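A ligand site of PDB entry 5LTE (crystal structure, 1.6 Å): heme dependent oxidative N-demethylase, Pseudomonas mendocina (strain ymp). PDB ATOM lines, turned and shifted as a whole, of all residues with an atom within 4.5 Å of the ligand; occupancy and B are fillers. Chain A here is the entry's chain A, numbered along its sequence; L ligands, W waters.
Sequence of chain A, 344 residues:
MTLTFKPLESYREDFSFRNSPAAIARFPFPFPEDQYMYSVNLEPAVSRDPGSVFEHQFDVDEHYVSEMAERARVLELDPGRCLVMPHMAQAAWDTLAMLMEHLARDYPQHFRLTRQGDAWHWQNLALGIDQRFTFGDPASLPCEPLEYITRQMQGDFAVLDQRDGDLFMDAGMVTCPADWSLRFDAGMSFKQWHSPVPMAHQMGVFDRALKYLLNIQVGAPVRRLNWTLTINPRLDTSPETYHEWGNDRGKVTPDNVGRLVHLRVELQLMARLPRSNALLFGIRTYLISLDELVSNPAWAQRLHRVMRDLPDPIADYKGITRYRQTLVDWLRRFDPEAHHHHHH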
ATOM      1  N   TYR A  38      10.089  25.686 -29.144  1.00  0.00           N
ATOM      2  CA  TYR A  38      11.010  26.572 -28.468  1.00  0.00           C
ATOM      3  C   TYR A  38      10.633  28.060 -28.687  1.00  0.00           C
ATOM      4  O   TYR A  38      10.162  28.456 -29.790  1.00  0.00           O
ATOM      5  CB  TYR A  38      12.450  26.355 -29.015  1.00  0.00           C
ATOM      6  CG  TYR A  38      13.081  24.996 -28.763  1.00  0.00           C
ATOM      7  CD1 TYR A  38      12.938  24.309 -27.530  1.00  0.00           C
ATOM      8  CD2 TYR A  38      13.788  24.388 -29.727  1.00  0.00           C
ATOM      9  CE1 TYR A  38      13.528  23.078 -27.325  1.00  0.00           C
ATOM     10  CE2 TYR A  38      14.401  23.190 -29.543  1.00  0.00           C
ATOM     11  CZ  TYR A  38      14.307  22.536 -28.270  1.00  0.00           C
ATOM     12  OH  TYR A  38      14.988  21.372 -28.022  1.00  0.00           O
ATOM     13  N   SER A  39      10.897  28.872 -27.678  1.00  0.00           N
ATOM     14  CA  SER A  39      10.714  30.286 -27.689  1.00  0.00           C
ATOM     15  C   SER A  39      11.454  30.921 -26.573  1.00  0.00           C
ATOM     16  O   SER A  39      11.954  30.208 -25.681  1.00  0.00           O
ATOM     17  CB  SER A  39       9.224  30.604 -27.529  1.00  0.00           C
ATOM     18  OG  SER A  39       8.696  30.339 -26.247  1.00  0.00           O
ATOM     19  N   VAL A  40      11.548  32.242 -26.597  1.00  0.00           N
ATOM     20  CA  VAL A  40      12.042  33.005 -25.465  1.00  0.00           C
ATOM     21  C   VAL A  40      10.922  33.165 -24.477  1.00  0.00           C
ATOM     22  O   VAL A  40      10.189  34.188 -24.506  1.00  0.00           O
ATOM     23  CB  VAL A  40      12.721  34.325 -25.837  1.00  0.00           C
ATOM     24  CG1 VAL A  40      13.401  34.908 -24.607  1.00  0.00           C
ATOM     25  CG2 VAL A  40      13.855  34.047 -26.821  1.00  0.00           C
ATOM     26  N   ASN A  41      10.729  32.155 -23.645  1.00  0.00           N
ATOM     27  CA  ASN A  41       9.594  32.070 -22.762  1.00  0.00           C
ATOM     28  C   ASN A  41       9.839  32.609 -21.364  1.00  0.00           C
ATOM     29  O   ASN A  41       9.434  32.016 -20.355  1.00  0.00           O
ATOM     30  CB  ASN A  41       9.033  30.635 -22.740  1.00  0.00           C
ATOM     31  CG  ASN A  41      10.025  29.621 -22.232  1.00  0.00           C
ATOM     32  OD1 ASN A  41      11.198  29.825 -22.382  1.00  0.00           O
ATOM     33  ND2 ASN A  41       9.515  28.583 -21.619  1.00  0.00           N
ATOM     34  N   LEU A  42      10.553  33.725 -21.342  1.00  0.00           N
ATOM     35  CA  LEU A  42      10.933  34.382 -20.075  1.00  0.00           C
ATOM     36  C   LEU A  42       9.876  35.262 -19.535  1.00  0.00           C
ATOM     37  O   LEU A  42       9.094  35.869 -20.333  1.00  0.00           O
ATOM     38  CB  LEU A  42      12.168  35.171 -20.289  1.00  0.00           C
ATOM     39  CG  LEU A  42      13.458  34.399 -20.628  1.00  0.00           C
ATOM     40  CD1 LEU A  42      14.548  35.298 -21.155  1.00  0.00           C
ATOM     41  CD2 LEU A  42      13.945  33.639 -19.421  1.00  0.00           C
ATOM     42  N   ALA A 158      23.756  26.949 -11.668  1.00  0.00           N
ATOM     43  CA  ALA A 158      24.921  27.426 -12.267  1.00  0.00           C
ATOM     44  C   ALA A 158      25.118  28.866 -11.924  1.00  0.00           C
ATOM     45  O   ALA A 158      24.163  29.607 -11.661  1.00  0.00           O
ATOM     46  CB  ALA A 158      24.826  27.330 -13.790  1.00  0.00           C
ATOM     47  N   LEU A 160      27.094  32.185 -13.345  1.00  0.00           N
ATOM     48  CA  LEU A 160      27.688  32.673 -14.565  1.00  0.00           C
ATOM     49  C   LEU A 160      28.447  33.950 -14.361  1.00  0.00           C
ATOM     50  O   LEU A 160      27.886  34.926 -13.806  1.00  0.00           O
ATOM     51  CB  LEU A 160      26.585  32.953 -15.604  1.00  0.00           C
ATOM     52  CG  LEU A 160      25.712  31.740 -16.021  1.00  0.00           C
ATOM     53  CD1 LEU A 160      26.551  30.556 -16.361  1.00  0.00           C
ATOM     54  CD2 LEU A 160      24.580  31.407 -15.062  1.00  0.00           C
ATOM     55  N   LEU A 167      28.111  35.365 -21.095  1.00  0.00           N
ATOM     56  CA  LEU A 167      27.985  34.673 -19.811  1.00  0.00           C
ATOM     57  C   LEU A 167      28.803  33.418 -19.892  1.00  0.00           C
ATOM     58  O   LEU A 167      28.764  32.679 -20.905  1.00  0.00           O
ATOM     59  CB  LEU A 167      26.544  34.309 -19.520  1.00  0.00           C
ATOM     60  CG  LEU A 167      25.595  35.477 -19.352  1.00  0.00           C
ATOM     61  CD1 LEU A 167      24.159  35.013 -19.366  1.00  0.00           C
ATOM     62  CD2 LEU A 167      25.862  36.155 -18.031  1.00  0.00           C
ATOM     63  N   MET A 169      30.104  29.835 -17.831  1.00  0.00           N
ATOM     64  CA  MET A 169      29.680  28.852 -16.822  1.00  0.00           C
ATOM     65  C   MET A 169      30.870  28.493 -15.932  1.00  0.00           C
ATOM     66  O   MET A 169      31.575  27.517 -16.077  1.00  0.00           O
ATOM     67  CB  MET A 169      29.110  27.577 -17.462  1.00  0.00           C
ATOM     68  CG  MET A 169      28.381  26.773 -16.400  1.00  0.00           C
ATOM     69  SD  MET A 169      27.712  25.194 -16.990  1.00  0.00           S
ATOM     70  CE  MET A 169      26.521  25.728 -18.183  1.00  0.00           C
ATOM     71  N   ASP A 179      20.857  15.435 -18.654  1.00  0.00           N
ATOM     72  CA  ASP A 179      21.825  14.892 -19.592  1.00  0.00           C
ATOM     73  C   ASP A 179      22.803  15.925 -20.149  1.00  0.00           C
ATOM     74  O   ASP A 179      23.031  16.096 -21.357  1.00  0.00           O
ATOM     75  CB  ASP A 179      21.090  14.105 -20.740  1.00  0.00           C
ATOM     76  CG  ASP A 179      22.042  13.248 -21.501  1.00  0.00           C
ATOM     77  OD1 ASP A 179      23.158  12.890 -21.030  1.00  0.00           O
ATOM     78  OD2 ASP A 179      21.650  12.914 -22.655  1.00  0.00           O
ATOM     79  N   TRP A 180      23.521  16.533 -19.171  1.00  0.00           N
ATOM     80  CA  TRP A 180      24.626  17.438 -19.464  1.00  0.00           C
ATOM     81  C   TRP A 180      25.538  17.424 -18.223  1.00  0.00           C
ATOM     82  O   TRP A 180      25.102  16.824 -17.211  1.00  0.00           O
ATOM     83  CB  TRP A 180      24.237  18.879 -19.833  1.00  0.00           C
ATOM     84  CG  TRP A 180      23.507  19.649 -18.842  1.00  0.00           C
ATOM     85  CD1 TRP A 180      22.231  19.571 -18.564  1.00  0.00           C
ATOM     86  CD2 TRP A 180      24.074  20.582 -17.936  1.00  0.00           C
ATOM     87  NE1 TRP A 180      21.904  20.455 -17.525  1.00  0.00           N
ATOM     88  CE2 TRP A 180      23.003  21.102 -17.142  1.00  0.00           C
ATOM     89  CE3 TRP A 180      25.315  21.122 -17.812  1.00  0.00           C
ATOM     90  CZ2 TRP A 180      23.201  22.102 -16.220  1.00  0.00           C
ATOM     91  CZ3 TRP A 180      25.511  22.116 -16.862  1.00  0.00           C
ATOM     92  CH2 TRP A 180      24.453  22.592 -16.134  1.00  0.00           C
ATOM     93  N   ASP A 185      31.033  21.475 -19.385  1.00  0.00           N
ATOM     94  CA  ASP A 185      30.652  22.779 -19.819  1.00  0.00           C
ATOM     95  C   ASP A 185      31.383  23.909 -19.141  1.00  0.00           C
ATOM     96  O   ASP A 185      31.201  25.055 -19.514  1.00  0.00           O
ATOM     97  CB  ASP A 185      29.160  22.963 -19.740  1.00  0.00           C
ATOM     98  CG  ASP A 185      28.375  22.147 -20.753  1.00  0.00           C
ATOM     99  OD1 ASP A 185      28.906  21.230 -21.406  1.00  0.00           O
ATOM    100  OD2 ASP A 185      27.149  22.416 -20.838  1.00  0.00           O
ATOM    101  N   PHE A 190      27.682  31.228 -23.363  1.00  0.00           N
ATOM    102  CA  PHE A 190      26.243  30.988 -23.474  1.00  0.00           C
ATOM    103  C   PHE A 190      25.837  30.196 -24.751  1.00  0.00           C
ATOM    104  O   PHE A 190      25.106  29.199 -24.718  1.00  0.00           O
ATOM    105  CB  PHE A 190      25.493  32.281 -23.343  1.00  0.00           C
ATOM    106  CG  PHE A 190      23.960  32.137 -23.316  1.00  0.00           C
ATOM    107  CD1 PHE A 190      23.354  31.978 -22.141  1.00  0.00           C
ATOM    108  CD2 PHE A 190      23.146  32.223 -24.469  1.00  0.00           C
ATOM    109  CE1 PHE A 190      21.995  31.839 -22.028  1.00  0.00           C
ATOM    110  CE2 PHE A 190      21.740  32.116 -24.367  1.00  0.00           C
ATOM    111  CZ  PHE A 190      21.179  31.891 -23.159  1.00  0.00           C
ATOM    112  N   TRP A 193      27.702  26.476 -24.817  1.00  0.00           N
ATOM    113  CA  TRP A 193      27.080  25.372 -24.082  1.00  0.00           C
ATOM    114  C   TRP A 193      25.742  24.939 -24.647  1.00  0.00           C
ATOM    115  O   TRP A 193      25.334  23.802 -24.454  1.00  0.00           O
ATOM    116  CB  TRP A 193      27.033  25.613 -22.574  1.00  0.00           C
ATOM    117  CG  TRP A 193      26.056  26.464 -22.049  1.00  0.00           C
ATOM    118  CD1 TRP A 193      24.699  26.301 -22.122  1.00  0.00           C
ATOM    119  CD2 TRP A 193      26.250  27.711 -21.357  1.00  0.00           C
ATOM    120  NE1 TRP A 193      24.068  27.351 -21.535  1.00  0.00           N
ATOM    121  CE2 TRP A 193      24.990  28.227 -21.042  1.00  0.00           C
ATOM    122  CE3 TRP A 193      27.401  28.446 -20.921  1.00  0.00           C
ATOM    123  CZ2 TRP A 193      24.836  29.380 -20.302  1.00  0.00           C
ATOM    124  CZ3 TRP A 193      27.211  29.608 -20.247  1.00  0.00           C
ATOM    125  CH2 TRP A 193      25.962  30.088 -19.968  1.00  0.00           C
ATOM    126  N   HIS A 194      25.098  25.846 -25.347  1.00  0.00           N
ATOM    127  CA  HIS A 194      23.826  25.577 -26.039  1.00  0.00           C
ATOM    128  C   HIS A 194      24.007  24.979 -27.397  1.00  0.00           C
ATOM    129  O   HIS A 194      23.004  24.702 -28.062  1.00  0.00           O
ATOM    130  CB  HIS A 194      22.978  26.831 -26.113  1.00  0.00           C
ATOM    131  CG  HIS A 194      22.278  27.160 -24.839  1.00  0.00           C
ATOM    132  ND1 HIS A 194      22.405  28.372 -24.210  1.00  0.00           N
ATOM    133  CD2 HIS A 194      21.365  26.466 -24.116  1.00  0.00           C
ATOM    134  CE1 HIS A 194      21.549  28.444 -23.192  1.00  0.00           C
ATOM    135  NE2 HIS A 194      20.927  27.280 -23.108  1.00  0.00           N
ATOM    136  N   PRO A 196      24.465  22.018 -28.725  1.00  0.00           N
ATOM    137  CA  PRO A 196      23.762  20.801 -29.145  1.00  0.00           C
ATOM    138  C   PRO A 196      22.283  20.974 -29.415  1.00  0.00           C
ATOM    139  O   PRO A 196      21.682  20.041 -29.954  1.00  0.00           O
ATOM    140  CB  PRO A 196      23.960  19.849 -27.944  1.00  0.00           C
ATOM    141  CG  PRO A 196      25.060  20.454 -27.141  1.00  0.00           C
ATOM    142  CD  PRO A 196      25.013  21.897 -27.368  1.00  0.00           C
ATOM    143  N   VAL A 197      21.672  22.117 -29.052  1.00  0.00           N
ATOM    144  CA  VAL A 197      20.208  22.242 -29.136  1.00  0.00           C
ATOM    145  C   VAL A 197      19.813  22.461 -30.598  1.00  0.00           C
ATOM    146  O   VAL A 197      20.331  23.411 -31.238  1.00  0.00           O
ATOM    147  CB  VAL A 197      19.722  23.385 -28.234  1.00  0.00           C
ATOM    148  CG1 VAL A 197      18.241  23.522 -28.338  1.00  0.00           C
ATOM    149  CG2 VAL A 197      20.107  23.133 -26.787  1.00  0.00           C
ATOM    150  N   VAL A 205      16.564  32.259 -30.880  1.00  0.00           N
ATOM    151  CA  VAL A 205      16.114  32.129 -29.469  1.00  0.00           C
ATOM    152  C   VAL A 205      17.301  32.409 -28.550  1.00  0.00           C
ATOM    153  O   VAL A 205      17.190  33.128 -27.552  1.00  0.00           O
ATOM    154  CB  VAL A 205      15.519  30.730 -29.210  1.00  0.00           C
ATOM    155  CG1 VAL A 205      15.442  30.425 -27.780  1.00  0.00           C
ATOM    156  CG2 VAL A 205      14.107  30.678 -29.748  1.00  0.00           C
ATOM    157  N   PHE A 206      18.440  31.830 -28.887  1.00  0.00           N
ATOM    158  CA  PHE A 206      19.658  32.037 -28.039  1.00  0.00           C
ATOM    159  C   PHE A 206      20.226  33.461 -28.172  1.00  0.00           C
ATOM    160  O   PHE A 206      20.650  34.052 -27.170  1.00  0.00           O
ATOM    161  CB  PHE A 206      20.703  30.982 -28.204  1.00  0.00           C
ATOM    162  CG  PHE A 206      20.221  29.632 -27.794  1.00  0.00           C
ATOM    163  CD1 PHE A 206      19.844  29.391 -26.511  1.00  0.00           C
ATOM    164  CD2 PHE A 206      20.198  28.593 -28.661  1.00  0.00           C
ATOM    165  CE1 PHE A 206      19.358  28.189 -26.077  1.00  0.00           C
ATOM    166  CE2 PHE A 206      19.711  27.365 -28.247  1.00  0.00           C
ATOM    167  CZ  PHE A 206      19.267  27.177 -26.964  1.00  0.00           C
ATOM    168  N   ALA A 209      17.749  35.522 -26.075  1.00  0.00           N
ATOM    169  CA  ALA A 209      17.800  35.164 -24.654  1.00  0.00           C
ATOM    170  C   ALA A 209      19.019  35.767 -23.988  1.00  0.00           C
ATOM    171  O   ALA A 209      18.894  36.301 -22.909  1.00  0.00           O
ATOM    172  CB  ALA A 209      17.776  33.590 -24.512  1.00  0.00           C
ATOM    173  N   LEU A 213      19.127  38.253 -20.753  1.00  0.00           N
ATOM    174  CA  LEU A 213      19.850  37.862 -19.514  1.00  0.00           C
ATOM    175  C   LEU A 213      20.956  38.883 -19.121  1.00  0.00           C
ATOM    176  O   LEU A 213      21.160  39.139 -17.911  1.00  0.00           O
ATOM    177  CB  LEU A 213      20.423  36.438 -19.650  1.00  0.00           C
ATOM    178  CG  LEU A 213      19.477  35.405 -19.126  1.00  0.00           C
ATOM    179  CD1 LEU A 213      18.123  35.504 -19.831  1.00  0.00           C
ATOM    180  CD2 LEU A 213      20.118  34.077 -19.309  1.00  0.00           C
ATOM    181  N   ARG A 224      11.819  30.971 -16.462  1.00  0.00           N
ATOM    182  CA  ARG A 224      11.143  30.232 -17.545  1.00  0.00           C
ATOM    183  C   ARG A 224      11.007  28.764 -17.142  1.00  0.00           C
ATOM    184  O   ARG A 224      11.604  28.326 -16.162  1.00  0.00           O
ATOM    185  CB  ARG A 224      11.930  30.257 -18.830  1.00  0.00           C
ATOM    186  CG  ARG A 224      13.330  29.548 -18.813  1.00  0.00           C
ATOM    187  CD  ARG A 224      14.025  29.470 -20.142  1.00  0.00           C
ATOM    188  NE  ARG A 224      13.456  28.605 -21.128  1.00  0.00           N
ATOM    189  CZ  ARG A 224      13.877  27.369 -21.401  1.00  0.00           C
ATOM    190  NH1 ARG A 224      14.795  26.793 -20.666  1.00  0.00           N
ATOM    191  NH2 ARG A 224      13.346  26.674 -22.376  1.00  0.00           N
ATOM    192  N   ASN A 226      11.453  24.790 -18.569  1.00  0.00           N
ATOM    193  CA  ASN A 226      11.963  23.830 -19.552  1.00  0.00           C
ATOM    194  C   ASN A 226      11.342  22.482 -19.159  1.00  0.00           C
ATOM    195  O   ASN A 226      10.799  22.305 -18.042  1.00  0.00           O
ATOM    196  CB  ASN A 226      13.505  23.663 -19.617  1.00  0.00           C
ATOM    197  CG  ASN A 226      13.893  23.082 -20.918  1.00  0.00           C
ATOM    198  OD1 ASN A 226      13.642  23.742 -21.969  1.00  0.00           O
ATOM    199  ND2 ASN A 226      14.436  21.833 -20.917  1.00  0.00           N
ATOM    200  N   TRP A 227      11.394  21.498 -20.059  1.00  0.00           N
ATOM    201  CA  TRP A 227      10.811  20.183 -19.758  1.00  0.00           C
ATOM    202  C   TRP A 227      11.555  19.156 -20.535  1.00  0.00           C
ATOM    203  O   TRP A 227      12.225  19.409 -21.554  1.00  0.00           O
ATOM    204  CB  TRP A 227       9.351  20.101 -20.053  1.00  0.00           C
ATOM    205  CG  TRP A 227       9.087  20.117 -21.536  1.00  0.00           C
ATOM    206  CD1 TRP A 227       9.032  21.235 -22.327  1.00  0.00           C
ATOM    207  CD2 TRP A 227       8.891  18.991 -22.412  1.00  0.00           C
ATOM    208  NE1 TRP A 227       8.826  20.837 -23.612  1.00  0.00           N
ATOM    209  CE2 TRP A 227       8.780  19.508 -23.723  1.00  0.00           C
ATOM    210  CE3 TRP A 227       8.843  17.579 -22.245  1.00  0.00           C
ATOM    211  CZ2 TRP A 227       8.533  18.689 -24.835  1.00  0.00           C
ATOM    212  CZ3 TRP A 227       8.665  16.743 -23.354  1.00  0.00           C
ATOM    213  CH2 TRP A 227       8.495  17.315 -24.643  1.00  0.00           C
ATOM    214  N   MET A 270      16.663  33.192 -13.131  1.00  0.00           N
ATOM    215  CA  MET A 270      17.828  33.951 -13.363  1.00  0.00           C
ATOM    216  C   MET A 270      17.805  35.233 -12.535  1.00  0.00           C
ATOM    217  O   MET A 270      16.913  36.069 -12.710  1.00  0.00           O
ATOM    218  CB  MET A 270      17.933  34.331 -14.840  1.00  0.00           C
ATOM    219  CG  MET A 270      18.144  33.084 -15.756  1.00  0.00           C
ATOM    220  SD  MET A 270      17.033  32.858 -17.195  1.00  0.00           S
ATOM    221  CE  MET A 270      15.614  32.208 -16.363  1.00  0.00           C
ATOM    222  N   PHE A 281      21.739  31.002 -11.939  1.00  0.00           N
ATOM    223  CA  PHE A 281      20.781  30.237 -12.730  1.00  0.00           C
ATOM    224  C   PHE A 281      20.347  29.040 -11.870  1.00  0.00           C
ATOM    225  O   PHE A 281      21.160  28.117 -11.617  1.00  0.00           O
ATOM    226  CB  PHE A 281      21.443  29.776 -13.992  1.00  0.00           C
ATOM    227  CG  PHE A 281      20.518  28.997 -14.986  1.00  0.00           C
ATOM    228  CD1 PHE A 281      19.446  29.666 -15.596  1.00  0.00           C
ATOM    229  CD2 PHE A 281      20.771  27.717 -15.333  1.00  0.00           C
ATOM    230  CE1 PHE A 281      18.674  29.001 -16.540  1.00  0.00           C
ATOM    231  CE2 PHE A 281      19.960  27.046 -16.310  1.00  0.00           C
ATOM    232  CZ  PHE A 281      18.925  27.710 -16.867  1.00  0.00           C
ATOM    233  N   TYR A 317      16.511  15.198 -29.556  1.00  0.00           N
ATOM    234  CA  TYR A 317      17.357  15.935 -28.620  1.00  0.00           C
ATOM    235  C   TYR A 317      17.019  15.611 -27.200  1.00  0.00           C
ATOM    236  O   TYR A 317      17.979  15.415 -26.386  1.00  0.00           O
ATOM    237  CB  TYR A 317      17.306  17.475 -28.862  1.00  0.00           C
ATOM    238  CG  TYR A 317      17.939  18.223 -27.716  1.00  0.00           C
ATOM    239  CD1 TYR A 317      19.318  18.367 -27.689  1.00  0.00           C
ATOM    240  CD2 TYR A 317      17.196  18.660 -26.631  1.00  0.00           C
ATOM    241  CE1 TYR A 317      19.937  18.961 -26.598  1.00  0.00           C
ATOM    242  CE2 TYR A 317      17.815  19.246 -25.535  1.00  0.00           C
ATOM    243  CZ  TYR A 317      19.194  19.352 -25.532  1.00  0.00           C
ATOM    244  OH  TYR A 317      19.768  19.952 -24.363  1.00  0.00           O
ATOM    245  N   LYS A 318      15.730  15.534 -26.886  1.00  0.00           N
ATOM    246  CA  LYS A 318      15.277  15.256 -25.522  1.00  0.00           C
ATOM    247  C   LYS A 318      15.437  13.798 -25.044  1.00  0.00           C
ATOM    248  O   LYS A 318      15.196  13.516 -23.861  1.00  0.00           O
ATOM    249  CB  LYS A 318      13.821  15.692 -25.341  1.00  0.00           C
ATOM    250  CG  LYS A 318      13.576  17.226 -25.396  1.00  0.00           C
ATOM    251  CD  LYS A 318      12.150  17.658 -25.366  1.00  0.00           C
ATOM    252  CE  LYS A 318      11.989  19.181 -25.482  1.00  0.00           C
ATOM    253  NZ  LYS A 318      12.251  19.880 -24.222  1.00  0.00           N
HETATM  254  C1  LIG L   1      19.485  23.504 -22.980  1.00  0.00           C
HETATM  255  C2  LIG L   1      22.180  25.838 -19.677  1.00  0.00           C
HETATM  256  C3  LIG L   1      19.376  29.855 -20.227  1.00  0.00           C
HETATM  257  C4  LIG L   1      16.831  27.516 -23.664  1.00  0.00           C
HETATM  258  C5  LIG L   1      20.486  23.831 -22.086  1.00  0.00           C
HETATM  259  C6  LIG L   1      21.519  22.918 -21.677  1.00  0.00           C
HETATM  260  C7  LIG L   1      22.285  23.630 -20.753  1.00  0.00           C
HETATM  261  C8  LIG L   1      21.694  24.926 -20.595  1.00  0.00           C
HETATM  262  C9  LIG L   1      23.565  23.219 -20.063  1.00  0.00           C
HETATM  263  C10 LIG L   1      21.787  21.565 -22.154  1.00  0.00           C
HETATM  264  C11 LIG L   1      22.594  21.575 -23.441  1.00  0.00           C
HETATM  265  C12 LIG L   1      23.070  20.199 -23.741  1.00  0.00           C
HETATM  266  O1  LIG L   1      24.241  19.807 -23.520  1.00  0.00           O
HETATM  267  O2  LIG L   1      22.255  19.359 -24.312  1.00  0.00           O
HETATM  268  C13 LIG L   1      21.585  27.087 -19.501  1.00  0.00           C
HETATM  269  C14 LIG L   1      22.075  28.102 -18.590  1.00  0.00           C
HETATM  270  C15 LIG L   1      21.320  29.238 -18.799  1.00  0.00           C
HETATM  271  C16 LIG L   1      20.288  28.922 -19.809  1.00  0.00           C
HETATM  272  C17 LIG L   1      23.263  27.973 -17.658  1.00  0.00           C
HETATM  273  C18 LIG L   1      21.461  30.598 -18.122  1.00  0.00           C
HETATM  274  C19 LIG L   1      22.618  31.141 -17.931  1.00  0.00           C
HETATM  275  C20 LIG L   1      18.445  29.604 -21.215  1.00  0.00           C
HETATM  276  C21 LIG L   1      17.443  30.514 -21.644  1.00  0.00           C
HETATM  277  C22 LIG L   1      16.726  29.856 -22.662  1.00  0.00           C
HETATM  278  C23 LIG L   1      17.274  28.515 -22.804  1.00  0.00           C
HETATM  279  C24 LIG L   1      17.272  31.861 -21.124  1.00  0.00           C
HETATM  280  C25 LIG L   1      15.597  30.489 -23.357  1.00  0.00           C
HETATM  281  C26 LIG L   1      14.865  29.824 -24.144  1.00  0.00           C
HETATM  282  C27 LIG L   1      17.368  26.279 -23.719  1.00  0.00           C
HETATM  283  C28 LIG L   1      16.803  25.256 -24.579  1.00  0.00           C
HETATM  284  C29 LIG L   1      17.507  24.081 -24.383  1.00  0.00           C
HETATM  285  C30 LIG L   1      18.551  24.413 -23.382  1.00  0.00           C
HETATM  286  C31 LIG L   1      15.579  25.480 -25.479  1.00  0.00           C
HETATM  287  C32 LIG L   1      17.159  22.711 -24.954  1.00  0.00           C
HETATM  288  C33 LIG L   1      16.264  22.073 -23.862  1.00  0.00           C
HETATM  289  C34 LIG L   1      15.303  20.969 -24.233  1.00  0.00           C
HETATM  290  O3  LIG L   1      14.971  20.805 -25.411  1.00  0.00           O
HETATM  291  O4  LIG L   1      14.846  20.217 -23.313  1.00  0.00           O
HETATM  292  N1  LIG L   1      20.579  25.033 -21.403  1.00  0.00           N
HETATM  293  N2  LIG L   1      20.556  27.657 -20.224  1.00  0.00           N
HETATM  294  N3  LIG L   1      18.354  28.386 -21.923  1.00  0.00           N
HETATM  295  N4  LIG L   1      18.433  25.764 -23.054  1.00  0.00           N
HETATM  296 FE1  LIG L   1      19.491  26.693 -21.676  1.00  0.00          FE
HETATM  297  O   HOH W   1      24.875  17.114 -23.362  1.00  0.00           O
HETATM  298  O   HOH W   2      26.072  21.577 -23.083  1.00  0.00           O
HETATM  299  O   HOH W   3      23.174  17.249 -26.088  1.00  0.00           O
HETATM  300  O   HOH W   4      12.231  22.627 -24.060  1.00  0.00           O
HETATM  301  O   HOH W   5      20.993  16.967 -23.165  1.00  0.00           O
HETATM  302  O   HOH W   6      16.156  18.805 -21.505  1.00  0.00           O
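The side-chain amino group (NZ) of Lys 318 lies within salt-bridge range of an oxygen (O4) of the ligand.
OH of Tyr 38 is in hydrogen-bond range of O3 of the ligand (2.7 Å).
A ring nitrogen (NE2) of His 194 binds an iron atom (FE1) of the ligand (2.1 Å).
The side-chain hydroxyl of Tyr 317 sits at hydrogen-bond distance from an oxygen (O2) of the ligand (2.6 Å).
The side-chain amide nitrogen of Asn 226 is in hydrogen-bond range of an oxygen (O4) of the ligand (2.9 Å).
NE of Arg 224 lies within hydrogen-bond range of OD1 of Asn 41 (2.9 Å).
O of Ser 39 sits close to OD1 of Asn 41, 3.4 Å away.
A ring nitrogen (ND1) of His 194 lies within hydrogen-bond range of the backbone carbonyl oxygen (O) of Phe 190.
The side-chain amino group (NZ) of Lys 318 sits at hydrogen-bond distance from the backbone carbonyl oxygen (O) of Trp 227 (2.7 Å).
O of Ala 158 sits at hydrogen-bond distance from N of Phe 281.
N of Phe 190 is in hydrogen-bond range of O of Leu 167 (3.1 Å).
ND1 of His 194 lies close to NE1 of Trp 193, 3.3 Å away.
OD1 of Asn 226 sits at hydrogen-bond distance from NH2 of Arg 224, at 3.0 Å.
O4 of the ligand lies close to O of Trp 227, 3.3 Å away.
Residues that only touch the ligand: Trp 193, Phe 281, Ser 39, Trp 180, Leu 160, Val 197, Arg 224, Phe 206, Val 205, Phe 190, Asp 185, Pro 196, Ala 209, Leu 213 and Met 169.
The nearest printed residue that does not touch the ligand is Met 270 (4.1 Å).
Water W2 lies within hydrogen-bond range of an oxygen (O1) of the ligand (2.6 Å), the side-chain carboxylate of Asp 185 (2.6 Å) and the backbone carbonyl oxygen of Trp 193 (2.7 Å).
Water W1 bridges O1 of the ligand and O of Asp 179.
Water W5 lies within hydrogen-bond range of O of Asp 179, O2 of the ligand and OH of Tyr 317.
Water W4 bridges NZ of Lys 318 and OD1 of Asn 226.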
